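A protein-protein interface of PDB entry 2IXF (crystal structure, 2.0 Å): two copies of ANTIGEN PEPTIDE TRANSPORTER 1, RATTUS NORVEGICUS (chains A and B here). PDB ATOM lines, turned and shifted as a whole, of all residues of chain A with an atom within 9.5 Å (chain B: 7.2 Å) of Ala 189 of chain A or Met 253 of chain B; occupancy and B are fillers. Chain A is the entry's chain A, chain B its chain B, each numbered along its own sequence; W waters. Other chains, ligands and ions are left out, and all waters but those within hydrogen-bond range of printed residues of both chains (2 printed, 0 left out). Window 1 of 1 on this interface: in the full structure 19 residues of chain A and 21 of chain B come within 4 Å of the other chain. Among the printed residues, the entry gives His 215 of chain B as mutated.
Water W1 bridges OE1 of Gln 216 of chain A and O of His 215 of chain B. Water W2 bridges N of Ala 189 of chain A (2.9 Å) and ND1 of His 215 of chain B (3.0 Å).
The side-chain amide nitrogen (ND2) of Asn 54 of chain B sits at hydrogen-bond distance from the backbone carbonyl oxygen (O) of Ala 186 of chain A (2.9 Å). The backbone NH of Asn 54 of chain B lies within hydrogen-bond range of the side-chain carboxylate of Asp 188 of chain A (2.8 Å). The side-chain amide oxygen (OD1) of Asn 54 of chain B sits at hydrogen-bond distance from the side-chain amide nitrogen (ND2) of Asn 191 of chain A (2.8 Å).
Printed residues of chain A within 4 Å of Met 253 of chain B: Ala 189 (3.6 Å). No residue of chain A comes within 4 Å of Ser 252 of chain B. No residue of chain A comes within 4 Å of Val 254 of chain B. Of the printed residues of chain A, His 215 of chain B touches Ala 186, Leu 187 and Asp 188. Printed residues of chain A within 4 Å of Pro 53 of chain B: Asp 188 (3.4 Å). Of the printed residues of chain B, Asp 188 of chain A touches Pro 53, Asn 54 and His 215. Of the printed residues of chain A, Asn 54 of chain B touches Ala 186, Leu 187, Asp 188 and Asn 191. Printed residues of chain B within 4 Å of Leu 187 of chain A: Asn 54 (3.6 Å) and His 215 (3.9 Å). The nearest residue of chain A that does not touch Met 253 of chain B is Gly 190 of chain A (6.2 Å). The nearest printed residue of chain B that does not touch Asp 188 of chain A is Gly 52 of chain B (4.5 Å).
The side-chain carboxylate of Asp 188 of chain A is in hydrogen-bond range of the backbone NH of Gly 190 of chain A, at 3.3 Å. The side-chain carboxylate of Asp 188 of chain A is in hydrogen-bond range of the backbone NH of Asn 191 of chain A, 2.8 Å away. ND2 of Asn 54 of chain B lies within hydrogen-bond range of NE2 of His 215 of chain B, at 3.5 Å.
Of the 20 printed residues of chain B, 4 touch a printed residue of chain A. Hydrophobic or aromatic side chains of chain B within 4 Å of the printed part of chain A: Pro 53, His 215 and Met 253. Of the 20 printed residues of chain A, 5 touch a printed residue of chain B.
Position printed for both chains: 216. Of the 9 pairs that touch across the chains among the printed residues, none has its exchanged pair printed and touching as well.
Among the printed residues, merely in contact across the chains: Ala 186 of chain A with His 215 of chain B, Leu 187 of chain A with Asn 54 of chain B, Leu 187 of chain A with His 215 of chain B, Asp 188 of chain A with Pro 53 of chain B, Asp 188 of chain A with His 215 of chain B and Ala 189 of chain A with Met 253 of chain B.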
ATOM      1  N   GLU A 132      30.740 -23.266  -4.812  1.00  0.00           N
ATOM      2  CA  GLU A 132      30.343 -21.871  -4.598  1.00  0.00           C
ATOM      3  C   GLU A 132      31.274 -20.886  -5.300  1.00  0.00           C
ATOM      4  O   GLU A 132      30.813 -19.881  -5.849  1.00  0.00           O
ATOM      5  CB  GLU A 132      30.275 -21.544  -3.101  1.00  0.00           C
ATOM      6  CG  GLU A 132      29.159 -22.262  -2.341  1.00  0.00           C
ATOM      7  CD  GLU A 132      27.771 -21.921  -2.848  1.00  0.00           C
ATOM      8  OE1 GLU A 132      27.581 -20.809  -3.378  1.00  0.00           O
ATOM      9  OE2 GLU A 132      26.858 -22.763  -2.704  1.00  0.00           O
ATOM     10  N   SER A 133      32.576 -21.163  -5.277  1.00  0.00           N
ATOM     11  CA  SER A 133      33.563 -20.252  -5.872  1.00  0.00           C
ATOM     12  C   SER A 133      33.708 -20.450  -7.384  1.00  0.00           C
ATOM     13  O   SER A 133      34.276 -19.598  -8.071  1.00  0.00           O
ATOM     14  CB  SER A 133      34.924 -20.424  -5.192  1.00  0.00           C
ATOM     15  OG  SER A 133      35.481 -21.683  -5.492  1.00  0.00           O
ATOM     16  N   THR A 184      37.341 -10.871  -7.080  1.00  0.00           N
ATOM     17  CA  THR A 184      36.406 -11.433  -8.061  1.00  0.00           C
ATOM     18  C   THR A 184      36.493 -10.791  -9.448  1.00  0.00           C
ATOM     19  O   THR A 184      35.700 -11.111 -10.330  1.00  0.00           O
ATOM     20  CB  THR A 184      34.958 -11.329  -7.566  1.00  0.00           C
ATOM     21  OG1 THR A 184      34.626  -9.955  -7.343  1.00  0.00           O
ATOM     22  CG2 THR A 184      34.779 -12.122  -6.273  1.00  0.00           C
ATOM     23  N   SER A 185      37.457  -9.902  -9.654  1.00  0.00           N
ATOM     24  CA  SER A 185      37.606  -9.262 -10.957  1.00  0.00           C
ATOM     25  C   SER A 185      38.021 -10.266 -12.059  1.00  0.00           C
ATOM     26  O   SER A 185      37.717 -10.049 -13.228  1.00  0.00           O
ATOM     27  CB  SER A 185      38.570  -8.069 -10.873  1.00  0.00           C
ATOM     28  OG  SER A 185      39.867  -8.455 -10.463  1.00  0.00           O
ATOM     29  N   ALA A 186      38.670 -11.372 -11.684  1.00  0.00           N
ATOM     30  CA  ALA A 186      39.021 -12.439 -12.641  1.00  0.00           C
ATOM     31  C   ALA A 186      37.893 -13.458 -12.868  1.00  0.00           C
ATOM     32  O   ALA A 186      37.948 -14.256 -13.812  1.00  0.00           O
ATOM     33  CB  ALA A 186      40.302 -13.174 -12.188  1.00  0.00           C
ATOM     34  N   LEU A 187      36.878 -13.443 -12.007  1.00  0.00           N
ATOM     35  CA  LEU A 187      35.761 -14.373 -12.134  1.00  0.00           C
ATOM     36  C   LEU A 187      34.838 -13.956 -13.276  1.00  0.00           C
ATOM     37  O   LEU A 187      34.655 -12.767 -13.527  1.00  0.00           O
ATOM     38  CB  LEU A 187      34.967 -14.460 -10.822  1.00  0.00           C
ATOM     39  CG  LEU A 187      35.720 -15.069  -9.631  1.00  0.00           C
ATOM     40  CD1 LEU A 187      34.793 -15.225  -8.423  1.00  0.00           C
ATOM     41  CD2 LEU A 187      36.346 -16.412  -9.992  1.00  0.00           C
ATOM     42  N   ASP A 188      34.265 -14.940 -13.961  1.00  0.00           N
ATOM     43  CA  ASP A 188      33.266 -14.677 -15.003  1.00  0.00           C
ATOM     44  C   ASP A 188      31.921 -14.296 -14.384  1.00  0.00           C
ATOM     45  O   ASP A 188      31.753 -14.356 -13.168  1.00  0.00           O
ATOM     46  CB  ASP A 188      33.130 -15.854 -15.984  1.00  0.00           C
ATOM     47  CG  ASP A 188      32.631 -17.149 -15.337  1.00  0.00           C
ATOM     48  OD1 ASP A 188      31.897 -17.119 -14.327  1.00  0.00           O
ATOM     49  OD2 ASP A 188      32.981 -18.221 -15.873  1.00  0.00           O
ATOM     50  N   ALA A 189      30.976 -13.910 -15.237  1.00  0.00           N
ATOM     51  CA  ALA A 189      29.651 -13.452 -14.808  1.00  0.00           C
ATOM     52  C   ALA A 189      28.929 -14.445 -13.884  1.00  0.00           C
ATOM     53  O   ALA A 189      28.413 -14.060 -12.835  1.00  0.00           O
ATOM     54  CB  ALA A 189      28.787 -13.141 -16.037  1.00  0.00           C
ATOM     55  N   GLY A 190      28.907 -15.718 -14.267  1.00  0.00           N
ATOM     56  CA  GLY A 190      28.236 -16.739 -13.477  1.00  0.00           C
ATOM     57  C   GLY A 190      28.862 -16.947 -12.114  1.00  0.00           C
ATOM     58  O   GLY A 190      28.156 -17.044 -11.110  1.00  0.00           O
ATOM     59  N   ASN A 191      30.191 -17.009 -12.075  1.00  0.00           N
ATOM     60  CA  ASN A 191      30.915 -17.212 -10.820  1.00  0.00           C
ATOM     61  C   ASN A 191      30.813 -16.012  -9.872  1.00  0.00           C
ATOM     62  O   ASN A 191      30.634 -16.180  -8.667  1.00  0.00           O
ATOM     63  CB  ASN A 191      32.380 -17.560 -11.098  1.00  0.00           C
ATOM     64  CG  ASN A 191      32.540 -18.928 -11.738  1.00  0.00           C
ATOM     65  OD1 ASN A 191      31.718 -19.811 -11.531  1.00  0.00           O
ATOM     66  ND2 ASN A 191      33.599 -19.105 -12.519  1.00  0.00           N
ATOM     67  N   GLN A 192      30.929 -14.805 -10.420  1.00  0.00           N
ATOM     68  CA  GLN A 192      30.783 -13.591  -9.624  1.00  0.00           C
ATOM     69  C   GLN A 192      29.392 -13.517  -8.974  1.00  0.00           C
ATOM     70  O   GLN A 192      29.265 -13.226  -7.785  1.00  0.00           O
ATOM     71  CB  GLN A 192      31.032 -12.358 -10.492  1.00  0.00           C
ATOM     72  CG  GLN A 192      31.225 -11.086  -9.692  1.00  0.00           C
ATOM     73  CD  GLN A 192      31.852  -9.991 -10.519  1.00  0.00           C
ATOM     74  OE1 GLN A 192      33.050  -9.723 -10.407  1.00  0.00           O
ATOM     75  NE2 GLN A 192      31.054  -9.369 -11.383  1.00  0.00           N
ATOM     76  N   LEU A 193      28.366 -13.808  -9.767  1.00  0.00           N
ATOM     77  CA  LEU A 193      26.991 -13.844  -9.294  1.00  0.00           C
ATOM     78  C   LEU A 193      26.779 -14.836  -8.138  1.00  0.00           C
ATOM     79  O   LEU A 193      26.098 -14.508  -7.176  1.00  0.00           O
ATOM     80  CB  LEU A 193      26.046 -14.164 -10.456  1.00  0.00           C
ATOM     81  N   ARG A 194      27.376 -16.028  -8.228  1.00  0.00           N
ATOM     82  CA  ARG A 194      27.185 -17.059  -7.206  1.00  0.00           C
ATOM     83  C   ARG A 194      27.857 -16.686  -5.886  1.00  0.00           C
ATOM     84  O   ARG A 194      27.287 -16.900  -4.812  1.00  0.00           O
ATOM     85  CB  ARG A 194      27.698 -18.423  -7.689  1.00  0.00           C
ATOM     86  CG  ARG A 194      27.419 -19.559  -6.704  1.00  0.00           C
ATOM     87  CD  ARG A 194      27.196 -20.909  -7.390  1.00  0.00           C
ATOM     88  NE  ARG A 194      26.906 -21.967  -6.417  1.00  0.00           N
ATOM     89  CZ  ARG A 194      26.635 -23.234  -6.727  1.00  0.00           C
ATOM     90  NH1 ARG A 194      26.591 -23.632  -7.995  1.00  0.00           N
ATOM     91  NH2 ARG A 194      26.396 -24.112  -5.759  1.00  0.00           N
ATOM     92  N   VAL A 195      29.065 -16.139  -5.971  1.00  0.00           N
ATOM     93  CA  VAL A 195      29.795 -15.700  -4.784  1.00  0.00           C
ATOM     94  C   VAL A 195      29.004 -14.598  -4.059  1.00  0.00           C
ATOM     95  O   VAL A 195      28.899 -14.600  -2.843  1.00  0.00           O
ATOM     96  CB  VAL A 195      31.212 -15.215  -5.152  1.00  0.00           C
ATOM     97  CG1 VAL A 195      31.880 -14.512  -3.970  1.00  0.00           C
ATOM     98  CG2 VAL A 195      32.056 -16.402  -5.639  1.00  0.00           C
ATOM     99  N   GLN A 196      28.439 -13.675  -4.829  1.00  0.00           N
ATOM    100  CA  GLN A 196      27.628 -12.601  -4.269  1.00  0.00           C
ATOM    101  C   GLN A 196      26.373 -13.127  -3.580  1.00  0.00           C
ATOM    102  O   GLN A 196      26.045 -12.698  -2.475  1.00  0.00           O
ATOM    103  CB  GLN A 196      27.276 -11.576  -5.346  1.00  0.00           C
ATOM    104  CG  GLN A 196      28.461 -10.681  -5.700  1.00  0.00           C
ATOM    105  CD  GLN A 196      28.056  -9.516  -6.557  1.00  0.00           C
ATOM    106  OE1 GLN A 196      27.714  -8.446  -6.047  1.00  0.00           O
ATOM    107  NE2 GLN A 196      28.056  -9.719  -7.873  1.00  0.00           N
ATOM    108  N   ARG A 197      25.687 -14.075  -4.208  1.00  0.00           N
ATOM    109  CA  ARG A 197      24.538 -14.718  -3.563  1.00  0.00           C
ATOM    110  C   ARG A 197      24.923 -15.330  -2.219  1.00  0.00           C
ATOM    111  O   ARG A 197      24.199 -15.187  -1.243  1.00  0.00           O
ATOM    112  CB  ARG A 197      23.922 -15.784  -4.465  1.00  0.00           C
ATOM    113  CG  ARG A 197      23.094 -15.205  -5.592  1.00  0.00           C
ATOM    114  CD  ARG A 197      22.230 -16.255  -6.270  1.00  0.00           C
ATOM    115  NE  ARG A 197      22.951 -16.887  -7.372  1.00  0.00           N
ATOM    116  CZ  ARG A 197      23.506 -18.102  -7.355  1.00  0.00           C
ATOM    117  NH1 ARG A 197      23.438 -18.897  -6.279  1.00  0.00           N
ATOM    118  NH2 ARG A 197      24.134 -18.530  -8.448  1.00  0.00           N
ATOM    119  N   GLN A 216      34.726  -2.341  -9.712  1.00  0.00           N
ATOM    120  CA  GLN A 216      33.527  -2.744 -10.452  1.00  0.00           C
ATOM    121  C   GLN A 216      32.281  -2.130  -9.835  1.00  0.00           C
ATOM    122  O   GLN A 216      31.907  -2.480  -8.716  1.00  0.00           O
ATOM    123  CB  GLN A 216      33.374  -4.263 -10.444  1.00  0.00           C
ATOM    124  CG  GLN A 216      34.509  -5.003 -11.099  1.00  0.00           C
ATOM    125  CD  GLN A 216      34.241  -6.492 -11.191  1.00  0.00           C
ATOM    126  OE1 GLN A 216      33.428  -6.939 -12.008  1.00  0.00           O
ATOM    127  NE2 GLN A 216      34.917  -7.267 -10.351  1.00  0.00           N
ATOM    128  N   SER A 218      29.116  -2.554 -10.443  1.00  0.00           N
ATOM    129  CA  SER A 218      27.989  -3.464 -10.223  1.00  0.00           C
ATOM    130  C   SER A 218      28.083  -4.202  -8.890  1.00  0.00           C
ATOM    131  O   SER A 218      27.064  -4.517  -8.270  1.00  0.00           O
ATOM    132  CB  SER A 218      27.851  -4.458 -11.386  1.00  0.00           C
ATOM    133  OG  SER A 218      29.107  -5.010 -11.758  1.00  0.00           O
ATOM    134  N   LEU A 219      29.305  -4.461  -8.438  1.00  0.00           N
ATOM    135  CA  LEU A 219      29.505  -5.062  -7.129  1.00  0.00           C
ATOM    136  C   LEU A 219      29.320  -4.013  -6.026  1.00  0.00           C
ATOM    137  O   LEU A 219      28.704  -4.288  -5.000  1.00  0.00           O
ATOM    138  CB  LEU A 219      30.880  -5.722  -7.044  1.00  0.00           C
ATOM    139  CG  LEU A 219      31.256  -6.650  -8.207  1.00  0.00           C
ATOM    140  CD1 LEU A 219      32.439  -7.513  -7.816  1.00  0.00           C
ATOM    141  CD2 LEU A 219      30.084  -7.521  -8.646  1.00  0.00           C
ATOM    142  N   ARG A 222      25.569  -3.028  -4.984  1.00  0.00           N
ATOM    143  CA  ARG A 222      24.778  -3.977  -4.212  1.00  0.00           C
ATOM    144  C   ARG A 222      25.089  -3.942  -2.717  1.00  0.00           C
ATOM    145  O   ARG A 222      24.312  -4.449  -1.910  1.00  0.00           O
ATOM    146  CB  ARG A 222      25.011  -5.380  -4.761  1.00  0.00           C
ATOM    147  CG  ARG A 222      24.564  -5.519  -6.206  1.00  0.00           C
ATOM    148  CD  ARG A 222      24.858  -6.888  -6.757  1.00  0.00           C
ATOM    149  NE  ARG A 222      24.131  -7.937  -6.040  1.00  0.00           N
ATOM    150  CZ  ARG A 222      24.201  -9.233  -6.330  1.00  0.00           C
ATOM    151  NH1 ARG A 222      24.961  -9.654  -7.335  1.00  0.00           N
ATOM    152  NH2 ARG A 222      23.501 -10.114  -5.619  1.00  0.00           N
ATOM    153  N   VAL B  51      35.246 -12.089 -25.074  1.00  0.00           N
ATOM    154  CA  VAL B  51      34.584 -12.390 -23.804  1.00  0.00           C
ATOM    155  C   VAL B  51      34.239 -13.874 -23.741  1.00  0.00           C
ATOM    156  O   VAL B  51      34.194 -14.549 -24.770  1.00  0.00           O
ATOM    157  CB  VAL B  51      33.299 -11.533 -23.598  1.00  0.00           C
ATOM    158  CG1 VAL B  51      33.613 -10.034 -23.698  1.00  0.00           C
ATOM    159  CG2 VAL B  51      32.215 -11.906 -24.585  1.00  0.00           C
ATOM    160  N   GLY B  52      34.007 -14.380 -22.533  1.00  0.00           N
ATOM    161  CA  GLY B  52      33.650 -15.787 -22.342  1.00  0.00           C
ATOM    162  C   GLY B  52      33.968 -16.254 -20.934  1.00  0.00           C
ATOM    163  O   GLY B  52      34.698 -15.579 -20.217  1.00  0.00           O
ATOM    164  N   PRO B  53      33.426 -17.418 -20.529  1.00  0.00           N
ATOM    165  CA  PRO B  53      33.608 -17.918 -19.166  1.00  0.00           C
ATOM    166  C   PRO B  53      35.059 -18.206 -18.764  1.00  0.00           C
ATOM    167  O   PRO B  53      35.972 -18.221 -19.597  1.00  0.00           O
ATOM    168  CB  PRO B  53      32.797 -19.221 -19.154  1.00  0.00           C
ATOM    169  CG  PRO B  53      31.888 -19.142 -20.332  1.00  0.00           C
ATOM    170  CD  PRO B  53      32.606 -18.336 -21.343  1.00  0.00           C
ATOM    171  N   ASN B  54      35.251 -18.452 -17.480  1.00  0.00           N
ATOM    172  CA  ASN B  54      36.565 -18.796 -16.966  1.00  0.00           C
ATOM    173  C   ASN B  54      37.069 -20.077 -17.619  1.00  0.00           C
ATOM    174  O   ASN B  54      36.345 -21.072 -17.714  1.00  0.00           O
ATOM    175  CB  ASN B  54      36.544 -18.921 -15.435  1.00  0.00           C
ATOM    176  CG  ASN B  54      36.290 -17.590 -14.744  1.00  0.00           C
ATOM    177  OD1 ASN B  54      35.514 -17.508 -13.790  1.00  0.00           O
ATOM    178  ND2 ASN B  54      36.942 -16.539 -15.225  1.00  0.00           N
ATOM    179  N   THR B 214      38.197  -9.169 -21.794  1.00  0.00           N
ATOM    180  CA  THR B 214      37.596  -8.612 -20.569  1.00  0.00           C
ATOM    181  C   THR B 214      36.384  -9.394 -20.075  1.00  0.00           C
ATOM    182  O   THR B 214      35.686 -10.031 -20.865  1.00  0.00           O
ATOM    183  CB  THR B 214      37.177  -7.132 -20.796  1.00  0.00           C
ATOM    184  OG1 THR B 214      36.733  -6.541 -19.565  1.00  0.00           O
ATOM    185  CG2 THR B 214      36.071  -7.042 -21.835  1.00  0.00           C
ATOM    186  N   HIS B 215      36.160  -9.346 -18.759  1.00  0.00           N
ATOM    187  CA  HIS B 215      34.911  -9.801 -18.158  1.00  0.00           C
ATOM    188  C   HIS B 215      33.999  -8.602 -17.824  1.00  0.00           C
ATOM    189  O   HIS B 215      32.896  -8.792 -17.319  1.00  0.00           O
ATOM    190  CB  HIS B 215      35.168 -10.630 -16.886  1.00  0.00           C
ATOM    191  CG  HIS B 215      35.809 -11.963 -17.138  1.00  0.00           C
ATOM    192  ND1 HIS B 215      35.136 -13.020 -17.710  1.00  0.00           N
ATOM    193  CD2 HIS B 215      37.057 -12.417 -16.867  1.00  0.00           C
ATOM    194  CE1 HIS B 215      35.947 -14.061 -17.795  1.00  0.00           C
ATOM    195  NE2 HIS B 215      37.118 -13.723 -17.289  1.00  0.00           N
ATOM    196  N   GLN B 216      34.455  -7.382 -18.114  1.00  0.00           N
ATOM    197  CA  GLN B 216      33.672  -6.169 -17.839  1.00  0.00           C
ATOM    198  C   GLN B 216      32.744  -5.862 -19.014  1.00  0.00           C
ATOM    199  O   GLN B 216      33.199  -5.425 -20.071  1.00  0.00           O
ATOM    200  CB  GLN B 216      34.574  -4.959 -17.599  1.00  0.00           C
ATOM    201  CG  GLN B 216      35.707  -5.150 -16.605  1.00  0.00           C
ATOM    202  CD  GLN B 216      36.411  -3.838 -16.282  1.00  0.00           C
ATOM    203  OE1 GLN B 216      37.626  -3.712 -16.443  1.00  0.00           O
ATOM    204  NE2 GLN B 216      35.638  -2.848 -15.831  1.00  0.00           N
ATOM    205  N   LEU B 217      31.447  -6.074 -18.814  1.00  0.00           N
ATOM    206  CA  LEU B 217      30.445  -5.868 -19.863  1.00  0.00           C
ATOM    207  C   LEU B 217      30.444  -4.450 -20.449  1.00  0.00           C
ATOM    208  O   LEU B 217      30.242  -4.272 -21.647  1.00  0.00           O
ATOM    209  CB  LEU B 217      29.051  -6.210 -19.330  1.00  0.00           C
ATOM    210  N   ALA B 220      33.067  -4.281 -23.050  1.00  0.00           N
ATOM    211  CA  ALA B 220      32.682  -5.093 -24.211  1.00  0.00           C
ATOM    212  C   ALA B 220      31.640  -4.377 -25.073  1.00  0.00           C
ATOM    213  O   ALA B 220      31.762  -4.329 -26.297  1.00  0.00           O
ATOM    214  CB  ALA B 220      32.154  -6.447 -23.761  1.00  0.00           C
ATOM    215  N   ILE B 226      32.397  -8.076 -31.113  1.00  0.00           N
ATOM    216  CA  ILE B 226      32.550  -8.878 -29.900  1.00  0.00           C
ATOM    217  C   ILE B 226      32.617 -10.352 -30.271  1.00  0.00           C
ATOM    218  O   ILE B 226      31.796 -10.843 -31.023  1.00  0.00           O
ATOM    219  CB  ILE B 226      31.375  -8.673 -28.911  1.00  0.00           C
ATOM    220  CG1 ILE B 226      31.251  -7.202 -28.497  1.00  0.00           C
ATOM    221  CG2 ILE B 226      31.557  -9.538 -27.668  1.00  0.00           C
ATOM    222  CD1 ILE B 226      29.923  -6.873 -27.808  1.00  0.00           C
ATOM    223  N   PHE B 228      32.334 -14.023 -28.587  1.00  0.00           N
ATOM    224  CA  PHE B 228      32.005 -14.800 -27.397  1.00  0.00           C
ATOM    225  C   PHE B 228      32.650 -16.184 -27.478  1.00  0.00           C
ATOM    226  O   PHE B 228      32.240 -17.013 -28.282  1.00  0.00           O
ATOM    227  CB  PHE B 228      30.487 -14.926 -27.209  1.00  0.00           C
ATOM    228  CG  PHE B 228      30.097 -15.360 -25.828  1.00  0.00           C
ATOM    229  CD1 PHE B 228      30.116 -16.702 -25.474  1.00  0.00           C
ATOM    230  CD2 PHE B 228      29.752 -14.425 -24.865  1.00  0.00           C
ATOM    231  CE1 PHE B 228      29.779 -17.106 -24.195  1.00  0.00           C
ATOM    232  CE2 PHE B 228      29.411 -14.822 -23.579  1.00  0.00           C
ATOM    233  CZ  PHE B 228      29.429 -16.162 -23.243  1.00  0.00           C
ATOM    234  N   GLY B 248      21.327 -15.068 -27.372  1.00  0.00           N
ATOM    235  CA  GLY B 248      22.063 -16.277 -26.971  1.00  0.00           C
ATOM    236  C   GLY B 248      22.925 -16.099 -25.725  1.00  0.00           C
ATOM    237  O   GLY B 248      22.478 -15.520 -24.733  1.00  0.00           O
ATOM    238  N   CYS B 249      24.162 -16.597 -25.777  1.00  0.00           N
ATOM    239  CA  CYS B 249      25.046 -16.644 -24.602  1.00  0.00           C
ATOM    240  C   CYS B 249      25.465 -15.267 -24.090  1.00  0.00           C
ATOM    241  O   CYS B 249      25.591 -15.066 -22.883  1.00  0.00           O
ATOM    242  CB  CYS B 249      26.314 -17.451 -24.907  1.00  0.00           C
ATOM    243  SG  CYS B 249      26.066 -19.221 -25.170  1.00  0.00           S
ATOM    244  N   TYR B 250      25.705 -14.339 -25.015  1.00  0.00           N
ATOM    245  CA  TYR B 250      26.100 -12.977 -24.669  1.00  0.00           C
ATOM    246  C   TYR B 250      24.963 -12.216 -23.997  1.00  0.00           C
ATOM    247  O   TYR B 250      25.181 -11.538 -22.995  1.00  0.00           O
ATOM    248  CB  TYR B 250      26.564 -12.213 -25.913  1.00  0.00           C
ATOM    249  CG  TYR B 250      26.932 -10.773 -25.635  1.00  0.00           C
ATOM    250  CD1 TYR B 250      28.146 -10.446 -25.040  1.00  0.00           C
ATOM    251  CD2 TYR B 250      26.058  -9.736 -25.958  1.00  0.00           C
ATOM    252  CE1 TYR B 250      28.479  -9.126 -24.779  1.00  0.00           C
ATOM    253  CE2 TYR B 250      26.384  -8.418 -25.705  1.00  0.00           C
ATOM    254  CZ  TYR B 250      27.595  -8.117 -25.116  1.00  0.00           C
ATOM    255  OH  TYR B 250      27.918  -6.809 -24.862  1.00  0.00           O
ATOM    256  N   ARG B 251      23.758 -12.317 -24.555  1.00  0.00           N
ATOM    257  CA  ARG B 251      22.587 -11.690 -23.946  1.00  0.00           C
ATOM    258  C   ARG B 251      22.326 -12.263 -22.553  1.00  0.00           C
ATOM    259  O   ARG B 251      21.982 -11.522 -21.637  1.00  0.00           O
ATOM    260  CB  ARG B 251      21.342 -11.838 -24.832  1.00  0.00           C
ATOM    261  CG  ARG B 251      20.066 -11.257 -24.211  1.00  0.00           C
ATOM    262  CD  ARG B 251      19.202 -10.536 -25.234  1.00  0.00           C
ATOM    263  NE  ARG B 251      17.887 -10.183 -24.696  1.00  0.00           N
ATOM    264  CZ  ARG B 251      17.126  -9.166 -25.113  1.00  0.00           C
ATOM    265  NH1 ARG B 251      17.525  -8.347 -26.085  1.00  0.00           N
ATOM    266  NH2 ARG B 251      15.943  -8.959 -24.539  1.00  0.00           N
ATOM    267  N   SER B 252      22.498 -13.573 -22.397  1.00  0.00           N
ATOM    268  CA  SER B 252      22.320 -14.222 -21.094  1.00  0.00           C
ATOM    269  C   SER B 252      23.331 -13.703 -20.070  1.00  0.00           C
ATOM    270  O   SER B 252      22.989 -13.489 -18.909  1.00  0.00           O
ATOM    271  CB  SER B 252      22.435 -15.745 -21.219  1.00  0.00           C
ATOM    272  OG  SER B 252      21.358 -16.278 -21.972  1.00  0.00           O
ATOM    273  N   MET B 253      24.569 -13.501 -20.514  1.00  0.00           N
ATOM    274  CA  MET B 253      25.626 -12.942 -19.667  1.00  0.00           C
ATOM    275  C   MET B 253      25.287 -11.512 -19.231  1.00  0.00           C
ATOM    276  O   MET B 253      25.440 -11.160 -18.056  1.00  0.00           O
ATOM    277  CB  MET B 253      26.956 -12.957 -20.424  1.00  0.00           C
ATOM    278  CG  MET B 253      28.175 -12.626 -19.582  1.00  0.00           C
ATOM    279  SD  MET B 253      29.623 -12.302 -20.596  1.00  0.00           S
ATOM    280  CE  MET B 253      29.163 -10.754 -21.381  1.00  0.00           C
ATOM    281  N   VAL B 254      24.817 -10.701 -20.177  1.00  0.00           N
ATOM    282  CA  VAL B 254      24.446  -9.309 -19.906  1.00  0.00           C
ATOM    283  C   VAL B 254      23.274  -9.228 -18.933  1.00  0.00           C
ATOM    284  O   VAL B 254      23.282  -8.423 -18.001  1.00  0.00           O
ATOM    285  CB  VAL B 254      24.077  -8.561 -21.211  1.00  0.00           C
ATOM    286  CG1 VAL B 254      23.562  -7.162 -20.908  1.00  0.00           C
ATOM    287  CG2 VAL B 254      25.277  -8.496 -22.143  1.00  0.00           C
ATOM    288  N   GLU B 255      22.270 -10.071 -19.154  1.00  0.00           N
ATOM    289  CA  GLU B 255      21.077 -10.092 -18.316  1.00  0.00           C
ATOM    290  C   GLU B 255      21.298 -10.837 -16.995  1.00  0.00           C
ATOM    291  O   GLU B 255      20.520 -10.675 -16.055  1.00  0.00           O
ATOM    292  CB  GLU B 255      19.899 -10.675 -19.102  1.00  0.00           C
ATOM    293  CG  GLU B 255      19.507  -9.785 -20.285  1.00  0.00           C
ATOM    294  CD  GLU B 255      18.322 -10.300 -21.076  1.00  0.00           C
ATOM    295  OE1 GLU B 255      18.026 -11.512 -21.012  1.00  0.00           O
ATOM    296  OE2 GLU B 255      17.689  -9.479 -21.774  1.00  0.00           O
ATOM    297  N   ALA B 256      22.361 -11.635 -16.925  1.00  0.00           N
ATOM    298  CA  ALA B 256      22.763 -12.286 -15.679  1.00  0.00           C
ATOM    299  C   ALA B 256      23.424 -11.275 -14.749  1.00  0.00           C
ATOM    300  O   ALA B 256      22.835 -10.859 -13.752  1.00  0.00           O
ATOM    301  CB  ALA B 256      23.713 -13.439 -15.963  1.00  0.00           C
HETATM  302  O   HOH W   1      33.842  -8.169 -14.375  1.00  0.00           O
HETATM  303  O   HOH W   2      32.109 -13.214 -17.761  1.00  0.00           O
